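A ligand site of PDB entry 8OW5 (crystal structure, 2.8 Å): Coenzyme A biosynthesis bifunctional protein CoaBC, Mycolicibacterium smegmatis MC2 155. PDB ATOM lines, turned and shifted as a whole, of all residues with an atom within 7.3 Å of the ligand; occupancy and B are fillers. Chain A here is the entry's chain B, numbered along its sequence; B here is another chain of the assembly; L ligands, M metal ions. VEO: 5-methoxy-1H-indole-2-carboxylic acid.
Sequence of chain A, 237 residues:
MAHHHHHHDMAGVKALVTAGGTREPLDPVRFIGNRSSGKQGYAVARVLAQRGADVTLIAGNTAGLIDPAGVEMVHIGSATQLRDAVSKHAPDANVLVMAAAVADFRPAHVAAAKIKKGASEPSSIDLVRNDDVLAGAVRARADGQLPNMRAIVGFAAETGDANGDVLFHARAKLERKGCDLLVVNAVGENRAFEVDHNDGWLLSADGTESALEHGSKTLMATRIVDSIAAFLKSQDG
The side-chain amide nitrogen (NE2) of Gln 40 sits at hydrogen-bond distance from the backbone carbonyl oxygen (O) of Lys 217 (3.4 Å). The backbone NH (N) of Gly 38 lies within hydrogen-bond range of the side-chain hydroxyl (OG) of Ser 36. The side-chain hydroxyl (OG) of Ser 37 sits close to the backbone NH (N) of Lys 39 (3.3 Å). The backbone carbonyl oxygen of Val 29 of chain B sits at hydrogen-bond distance from the backbone NH of Arg 35, 3.2 Å away. The backbone NH (N) of Ala 101 lies within hydrogen-bond range of the backbone carbonyl oxygen (O) of Gly 20 (3.0 Å).
O14 of the ligand sits at hydrogen-bond distance from N of Gln 40 (2.8 Å). O13 of the ligand is in hydrogen-bond range of N of Gly 41 (3.1 Å). N07 of the ligand lies close to OG of Ser 36. An oxygen (O13) of the ligand sits close to the backbone NH (N) of Gly 38, 3.5 Å away. The side-chain hydroxyl of Ser 37 sits at hydrogen-bond distance from an oxygen (O14) of the ligand (3.2 Å). The backbone NH of Lys 39 is in hydrogen-bond range of an oxygen (O14) of the ligand, at 3.4 Å.
Residues that only touch the ligand: Ala 157 (3.7 Å), Val 187 (3.7 Å), Arg 35 (3.8 Å), Ala 101 (3.9 Å) and Val 29 of chain B (3.9 Å). Within 4 Å of the ligand: Arg 35, Ser 36, Ser 37, Gly 38, Lys 39, Gln 40, Gly 41, Ala 101, Ala 157, Val 187 and Val 29 of chain B.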
ATOM      1  N   THR A  18      17.552  -4.409  26.657  1.00  0.00           N
ATOM      2  CA  THR A  18      18.569  -5.124  27.411  1.00  0.00           C
ATOM      3  C   THR A  18      19.477  -5.887  26.451  1.00  0.00           C
ATOM      4  O   THR A  18      19.005  -6.469  25.464  1.00  0.00           O
ATOM      5  CB  THR A  18      17.910  -6.121  28.333  1.00  0.00           C
ATOM      6  OG1 THR A  18      17.741  -7.335  27.616  1.00  0.00           O
ATOM      7  CG2 THR A  18      16.534  -5.614  28.698  1.00  0.00           C
ATOM      8  N   ALA A  19      20.778  -5.900  26.727  1.00  0.00           N
ATOM      9  CA  ALA A  19      21.706  -6.491  25.778  1.00  0.00           C
ATOM     10  C   ALA A  19      22.934  -7.049  26.473  1.00  0.00           C
ATOM     11  O   ALA A  19      23.334  -6.572  27.540  1.00  0.00           O
ATOM     12  CB  ALA A  19      22.120  -5.474  24.710  1.00  0.00           C
ATOM     13  N   GLY A  20      23.542  -8.041  25.832  1.00  0.00           N
ATOM     14  CA  GLY A  20      24.686  -8.729  26.381  1.00  0.00           C
ATOM     15  C   GLY A  20      24.243  -9.941  27.149  1.00  0.00           C
ATOM     16  O   GLY A  20      23.062 -10.277  27.213  1.00  0.00           O
ATOM     17  N   GLY A  21      25.205 -10.616  27.754  1.00  0.00           N
ATOM     18  CA  GLY A  21      24.943 -11.821  28.521  1.00  0.00           C
ATOM     19  C   GLY A  21      25.330 -11.568  29.960  1.00  0.00           C
ATOM     20  O   GLY A  21      26.198 -10.742  30.231  1.00  0.00           O
ATOM     21  N   ASN A  34      26.459 -17.195  29.334  1.00  0.00           N
ATOM     22  CA  ASN A  34      25.785 -17.472  28.073  1.00  0.00           C
ATOM     23  C   ASN A  34      26.530 -16.683  26.998  1.00  0.00           C
ATOM     24  O   ASN A  34      27.106 -15.623  27.269  1.00  0.00           O
ATOM     25  CB  ASN A  34      24.259 -17.094  28.162  1.00  0.00           C
ATOM     26  CG  ASN A  34      23.417 -18.020  29.148  1.00  0.00           C
ATOM     27  OD1 ASN A  34      23.880 -18.410  30.224  1.00  0.00           O
ATOM     28  ND2 ASN A  34      22.161 -18.346  28.767  1.00  0.00           N
ATOM     29  N   ARG A  35      26.537 -17.186  25.757  1.00  0.00           N
ATOM     30  CA  ARG A  35      27.502 -16.758  24.757  1.00  0.00           C
ATOM     31  C   ARG A  35      27.095 -15.507  23.954  1.00  0.00           C
ATOM     32  O   ARG A  35      27.595 -15.350  22.825  1.00  0.00           O
ATOM     33  CB  ARG A  35      27.812 -17.893  23.787  1.00  0.00           C
ATOM     34  CG  ARG A  35      28.951 -18.812  24.225  1.00  0.00           C
ATOM     35  CD  ARG A  35      29.487 -19.619  23.064  1.00  0.00           C
ATOM     36  NE  ARG A  35      30.925 -19.869  23.179  1.00  0.00           N
ATOM     37  CZ  ARG A  35      31.460 -20.955  23.720  1.00  0.00           C
ATOM     38  NH1 ARG A  35      32.764 -21.188  23.664  1.00  0.00           N
ATOM     39  NH2 ARG A  35      30.671 -21.843  24.341  1.00  0.00           N
ATOM     40  N   SER A  36      26.242 -14.620  24.476  1.00  0.00           N
ATOM     41  CA  SER A  36      25.864 -13.444  23.704  1.00  0.00           C
ATOM     42  C   SER A  36      26.961 -12.386  23.681  1.00  0.00           C
ATOM     43  O   SER A  36      27.391 -11.897  24.733  1.00  0.00           O
ATOM     44  CB  SER A  36      24.591 -12.810  24.252  1.00  0.00           C
ATOM     45  OG  SER A  36      24.452 -11.491  23.757  1.00  0.00           O
ATOM     46  N   SER A  37      27.332 -11.939  22.472  1.00  0.00           N
ATOM     47  CA  SER A  37      28.314 -10.867  22.316  1.00  0.00           C
ATOM     48  C   SER A  37      27.693  -9.530  22.720  1.00  0.00           C
ATOM     49  O   SER A  37      28.415  -8.612  23.125  1.00  0.00           O
ATOM     50  CB  SER A  37      28.856 -10.799  20.884  1.00  0.00           C
ATOM     51  OG  SER A  37      27.858 -10.482  19.924  1.00  0.00           O
ATOM     52  N   GLY A  38      26.366  -9.422  22.610  1.00  0.00           N
ATOM     53  CA  GLY A  38      25.624  -8.183  22.764  1.00  0.00           C
ATOM     54  C   GLY A  38      25.496  -7.350  21.503  1.00  0.00           C
ATOM     55  O   GLY A  38      24.614  -6.498  21.430  1.00  0.00           O
ATOM     56  N   LYS A  39      26.285  -7.637  20.474  1.00  0.00           N
ATOM     57  CA  LYS A  39      26.313  -6.796  19.290  1.00  0.00           C
ATOM     58  C   LYS A  39      24.924  -6.642  18.675  1.00  0.00           C
ATOM     59  O   LYS A  39      24.522  -5.529  18.314  1.00  0.00           O
ATOM     60  CB  LYS A  39      27.273  -7.395  18.271  1.00  0.00           C
ATOM     61  CG  LYS A  39      28.708  -7.347  18.717  1.00  0.00           C
ATOM     62  CD  LYS A  39      29.640  -7.691  17.621  1.00  0.00           C
ATOM     63  CE  LYS A  39      30.893  -8.342  18.177  1.00  0.00           C
ATOM     64  NZ  LYS A  39      32.062  -7.410  18.106  1.00  0.00           N
ATOM     65  N   GLN A  40      24.172  -7.756  18.574  1.00  0.00           N
ATOM     66  CA  GLN A  40      22.842  -7.700  17.972  1.00  0.00           C
ATOM     67  C   GLN A  40      21.929  -6.791  18.766  1.00  0.00           C
ATOM     68  O   GLN A  40      21.176  -5.992  18.191  1.00  0.00           O
ATOM     69  CB  GLN A  40      22.233  -9.115  17.837  1.00  0.00           C
ATOM     70  CG  GLN A  40      20.913  -9.219  17.003  1.00  0.00           C
ATOM     71  CD  GLN A  40      20.919  -8.490  15.638  1.00  0.00           C
ATOM     72  OE1 GLN A  40      21.781  -8.744  14.792  1.00  0.00           O
ATOM     73  NE2 GLN A  40      19.952  -7.604  15.422  1.00  0.00           N
ATOM     74  N   GLY A  41      21.972  -6.876  20.101  1.00  0.00           N
ATOM     75  CA  GLY A  41      21.099  -6.018  20.881  1.00  0.00           C
ATOM     76  C   GLY A  41      21.478  -4.562  20.732  1.00  0.00           C
ATOM     77  O   GLY A  41      20.611  -3.701  20.538  1.00  0.00           O
ATOM     78  N   TYR A  42      22.776  -4.262  20.798  1.00  0.00           N
ATOM     79  CA  TYR A  42      23.229  -2.904  20.534  1.00  0.00           C
ATOM     80  C   TYR A  42      22.715  -2.414  19.189  1.00  0.00           C
ATOM     81  O   TYR A  42      22.184  -1.303  19.080  1.00  0.00           O
ATOM     82  CB  TYR A  42      24.770  -2.845  20.541  1.00  0.00           C
ATOM     83  CG  TYR A  42      25.502  -2.562  21.861  1.00  0.00           C
ATOM     84  CD1 TYR A  42      25.202  -3.233  23.032  1.00  0.00           C
ATOM     85  CD2 TYR A  42      26.547  -1.632  21.900  1.00  0.00           C
ATOM     86  CE1 TYR A  42      25.910  -2.973  24.204  1.00  0.00           C
ATOM     87  CE2 TYR A  42      27.234  -1.358  23.070  1.00  0.00           C
ATOM     88  CZ  TYR A  42      26.916  -2.033  24.212  1.00  0.00           C
ATOM     89  OH  TYR A  42      27.624  -1.733  25.351  1.00  0.00           O
ATOM     90  N   ALA A  43      22.715  -3.297  18.181  1.00  0.00           N
ATOM     91  CA  ALA A  43      22.402  -2.888  16.816  1.00  0.00           C
ATOM     92  C   ALA A  43      20.984  -2.355  16.686  1.00  0.00           C
ATOM     93  O   ALA A  43      20.747  -1.405  15.929  1.00  0.00           O
ATOM     94  CB  ALA A  43      22.612  -4.062  15.875  1.00  0.00           C
ATOM     95  N   THR A  62      29.466  -6.352  27.839  1.00  0.00           N
ATOM     96  CA  THR A  62      29.576  -6.231  26.436  1.00  0.00           C
ATOM     97  C   THR A  62      30.681  -5.302  26.206  1.00  0.00           C
ATOM     98  O   THR A  62      30.746  -4.694  25.169  1.00  0.00           O
ATOM     99  CB  THR A  62      28.428  -5.385  25.976  1.00  0.00           C
ATOM    100  OG1 THR A  62      28.189  -4.358  26.940  1.00  0.00           O
ATOM    101  CG2 THR A  62      27.196  -6.205  25.827  1.00  0.00           C
ATOM    102  N   ALA A  99      16.925  -8.374  24.282  1.00  0.00           N
ATOM    103  CA  ALA A  99      17.937  -9.061  23.503  1.00  0.00           C
ATOM    104  C   ALA A  99      19.068  -9.586  24.375  1.00  0.00           C
ATOM    105  O   ALA A  99      20.149  -9.896  23.864  1.00  0.00           O
ATOM    106  CB  ALA A  99      18.482  -8.131  22.420  1.00  0.00           C
ATOM    107  N   ALA A 100      18.882  -9.597  25.672  1.00  0.00           N
ATOM    108  CA  ALA A 100      19.893 -10.149  26.558  1.00  0.00           C
ATOM    109  C   ALA A 100      19.777 -11.670  26.637  1.00  0.00           C
ATOM    110  O   ALA A 100      18.667 -12.215  26.662  1.00  0.00           O
ATOM    111  CB  ALA A 100      19.750  -9.545  27.954  1.00  0.00           C
ATOM    112  N   ALA A 101      20.930 -12.338  26.637  1.00  0.00           N
ATOM    113  CA  ALA A 101      21.016 -13.771  26.935  1.00  0.00           C
ATOM    114  C   ALA A 101      21.202 -13.908  28.451  1.00  0.00           C
ATOM    115  O   ALA A 101      22.315 -13.980  28.968  1.00  0.00           O
ATOM    116  CB  ALA A 101      22.157 -14.427  26.171  1.00  0.00           C
ATOM    117  N   VAL A 102      20.057 -13.999  29.137  1.00  0.00           N
ATOM    118  CA  VAL A 102      20.036 -14.058  30.580  1.00  0.00           C
ATOM    119  C   VAL A 102      20.252 -15.435  31.133  1.00  0.00           C
ATOM    120  O   VAL A 102      19.704 -16.385  30.631  1.00  0.00           O
ATOM    121  CB  VAL A 102      18.684 -13.529  31.079  1.00  0.00           C
ATOM    122  CG1 VAL A 102      18.771 -13.043  32.504  1.00  0.00           C
ATOM    123  CG2 VAL A 102      18.152 -12.453  30.170  1.00  0.00           C
ATOM    124  N   PHE A 155      13.361 -12.363  22.307  1.00  0.00           N
ATOM    125  CA  PHE A 155      14.367 -12.928  21.408  1.00  0.00           C
ATOM    126  C   PHE A 155      14.580 -14.381  21.784  1.00  0.00           C
ATOM    127  O   PHE A 155      14.789 -14.690  22.956  1.00  0.00           O
ATOM    128  CB  PHE A 155      15.690 -12.210  21.529  1.00  0.00           C
ATOM    129  CG  PHE A 155      15.664 -10.862  20.972  1.00  0.00           C
ATOM    130  CD1 PHE A 155      15.025  -9.844  21.644  1.00  0.00           C
ATOM    131  CD2 PHE A 155      16.257 -10.615  19.750  1.00  0.00           C
ATOM    132  CE1 PHE A 155      14.997  -8.590  21.139  1.00  0.00           C
ATOM    133  CE2 PHE A 155      16.230  -9.341  19.222  1.00  0.00           C
ATOM    134  CZ  PHE A 155      15.591  -8.329  19.916  1.00  0.00           C
ATOM    135  N   ALA A 156      14.599 -15.261  20.804  1.00  0.00           N
ATOM    136  CA  ALA A 156      14.733 -16.661  21.144  1.00  0.00           C
ATOM    137  C   ALA A 156      15.826 -17.331  20.316  1.00  0.00           C
ATOM    138  O   ALA A 156      16.067 -17.000  19.151  1.00  0.00           O
ATOM    139  CB  ALA A 156      13.412 -17.386  20.952  1.00  0.00           C
ATOM    140  N   ALA A 157      16.478 -18.286  20.968  1.00  0.00           N
ATOM    141  CA  ALA A 157      17.405 -19.206  20.331  1.00  0.00           C
ATOM    142  C   ALA A 157      16.816 -20.600  20.473  1.00  0.00           C
ATOM    143  O   ALA A 157      16.427 -20.993  21.582  1.00  0.00           O
ATOM    144  CB  ALA A 157      18.782 -19.121  20.984  1.00  0.00           C
ATOM    145  N   GLU A 158      16.709 -21.317  19.350  1.00  0.00           N
ATOM    146  CA  GLU A 158      16.316 -22.727  19.329  1.00  0.00           C
ATOM    147  C   GLU A 158      17.137 -23.450  18.283  1.00  0.00           C
ATOM    148  O   GLU A 158      17.345 -22.919  17.188  1.00  0.00           O
ATOM    149  CB  GLU A 158      14.816 -22.901  19.037  1.00  0.00           C
ATOM    150  CG  GLU A 158      13.879 -22.107  19.957  1.00  0.00           C
ATOM    151  CD  GLU A 158      13.918 -22.561  21.430  1.00  0.00           C
ATOM    152  OE1 GLU A 158      14.740 -23.440  21.789  1.00  0.00           O
ATOM    153  OE2 GLU A 158      13.146 -22.027  22.249  1.00  0.00           O
ATOM    154  N   VAL A 187      20.416 -13.747  14.963  1.00  0.00           N
ATOM    155  CA  VAL A 187      21.673 -13.041  14.969  1.00  0.00           C
ATOM    156  C   VAL A 187      22.380 -13.367  13.713  1.00  0.00           C
ATOM    157  O   VAL A 187      22.410 -14.513  13.303  1.00  0.00           O
ATOM    158  CB  VAL A 187      22.532 -13.402  16.185  1.00  0.00           C
ATOM    159  CG1 VAL A 187      23.641 -12.390  16.395  1.00  0.00           C
ATOM    160  CG2 VAL A 187      21.687 -13.567  17.438  1.00  0.00           C
ATOM    161  N   GLY A 188      23.018 -12.393  13.106  1.00  0.00           N
ATOM    162  CA  GLY A 188      23.636 -12.538  11.813  1.00  0.00           C
ATOM    163  C   GLY A 188      25.156 -12.626  11.843  1.00  0.00           C
ATOM    164  O   GLY A 188      25.799 -12.649  12.886  1.00  0.00           O
ATOM    165  N   LYS A 217      23.814  -7.817  11.003  1.00  0.00           N
ATOM    166  CA  LYS A 217      23.187  -7.385  12.258  1.00  0.00           C
ATOM    167  C   LYS A 217      22.308  -6.154  12.066  1.00  0.00           C
ATOM    168  O   LYS A 217      21.281  -6.009  12.767  1.00  0.00           O
ATOM    169  CB  LYS A 217      24.279  -7.075  13.289  1.00  0.00           C
ATOM    170  CG  LYS A 217      24.692  -8.222  14.202  1.00  0.00           C
ATOM    171  CD  LYS A 217      26.171  -8.165  14.528  1.00  0.00           C
ATOM    172  CE  LYS A 217      26.683  -9.545  14.921  1.00  0.00           C
ATOM    173  NZ  LYS A 217      27.912  -9.909  14.165  1.00  0.00           N
ATOM    174  N   VAL B  29      25.708 -23.061  24.211  1.00  0.00           N
ATOM    175  CA  VAL B  29      25.406 -21.692  24.652  1.00  0.00           C
ATOM    176  C   VAL B  29      26.087 -21.365  25.980  1.00  0.00           C
ATOM    177  O   VAL B  29      26.749 -20.342  26.094  1.00  0.00           O
ATOM    178  CB  VAL B  29      23.891 -21.462  24.750  1.00  0.00           C
ATOM    179  CG1 VAL B  29      23.588 -20.391  25.785  1.00  0.00           C
ATOM    180  CG2 VAL B  29      23.326 -21.057  23.413  1.00  0.00           C
ATOM    181  N   ARG B  30      25.875 -22.196  26.986  1.00  0.00           N
ATOM    182  CA  ARG B  30      26.396 -21.933  28.322  1.00  0.00           C
ATOM    183  C   ARG B  30      27.814 -22.458  28.458  1.00  0.00           C
ATOM    184  O   ARG B  30      28.214 -23.405  27.769  1.00  0.00           O
ATOM    185  CB  ARG B  30      25.510 -22.581  29.376  1.00  0.00           C
ATOM    186  CG  ARG B  30      24.061 -22.166  29.279  1.00  0.00           C
ATOM    187  CD  ARG B  30      23.169 -23.320  29.462  1.00  0.00           C
ATOM    188  NE  ARG B  30      21.810 -22.955  29.096  1.00  0.00           N
ATOM    189  CZ  ARG B  30      20.717 -23.602  29.502  1.00  0.00           C
ATOM    190  NH1 ARG B  30      20.803 -24.655  30.301  1.00  0.00           N
ATOM    191  NH2 ARG B  30      19.530 -23.201  29.068  1.00  0.00           N
ATOM    192  N   LYS B 114      21.161 -27.329  22.622  1.00  0.00           N
ATOM    193  CA  LYS B 114      20.776 -26.566  23.779  1.00  0.00           C
ATOM    194  C   LYS B 114      19.943 -27.272  24.764  1.00  0.00           C
ATOM    195  O   LYS B 114      19.018 -27.976  24.435  1.00  0.00           O
ATOM    196  CB  LYS B 114      20.017 -25.357  23.317  1.00  0.00           C
ATOM    197  CG  LYS B 114      20.180 -24.127  24.188  1.00  0.00           C
ATOM    198  CD  LYS B 114      19.076 -23.128  23.891  1.00  0.00           C
ATOM    199  CE  LYS B 114      18.677 -22.404  25.145  1.00  0.00           C
ATOM    200  NZ  LYS B 114      18.117 -23.376  26.103  1.00  0.00           N
HETATM  201  C10 VEO L   1      22.459 -13.693  21.592  1.00  0.00           C
HETATM  202  C01 VEO L   1      21.752 -17.535  23.905  1.00  0.00           C
HETATM  203  C03 VEO L   1      22.006 -15.985  22.233  1.00  0.00           C
HETATM  204  C04 VEO L   1      23.265 -16.349  21.749  1.00  0.00           C
HETATM  205  C05 VEO L   1      24.112 -15.398  21.194  1.00  0.00           C
HETATM  206  C06 VEO L   1      23.698 -14.063  21.115  1.00  0.00           C
HETATM  207  C08 VEO L   1      23.510 -11.943  20.790  1.00  0.00           C
HETATM  208  C09 VEO L   1      22.330 -12.315  21.377  1.00  0.00           C
HETATM  209  C11 VEO L   1      21.602 -14.664  22.156  1.00  0.00           C
HETATM  210  C12 VEO L   1      23.850 -10.545  20.361  1.00  0.00           C
HETATM  211  N07 VEO L   1      24.311 -12.969  20.629  1.00  0.00           N
HETATM  212  O02 VEO L   1      21.169 -16.951  22.789  1.00  0.00           O
HETATM  213  O13 VEO L   1      23.293  -9.583  20.978  1.00  0.00           O
HETATM  214  O14 VEO L   1      24.654 -10.426  19.403  1.00  0.00           O
HETATM  215 CA    CA M   1      18.490 -19.876  28.917  1.00  0.00          CA
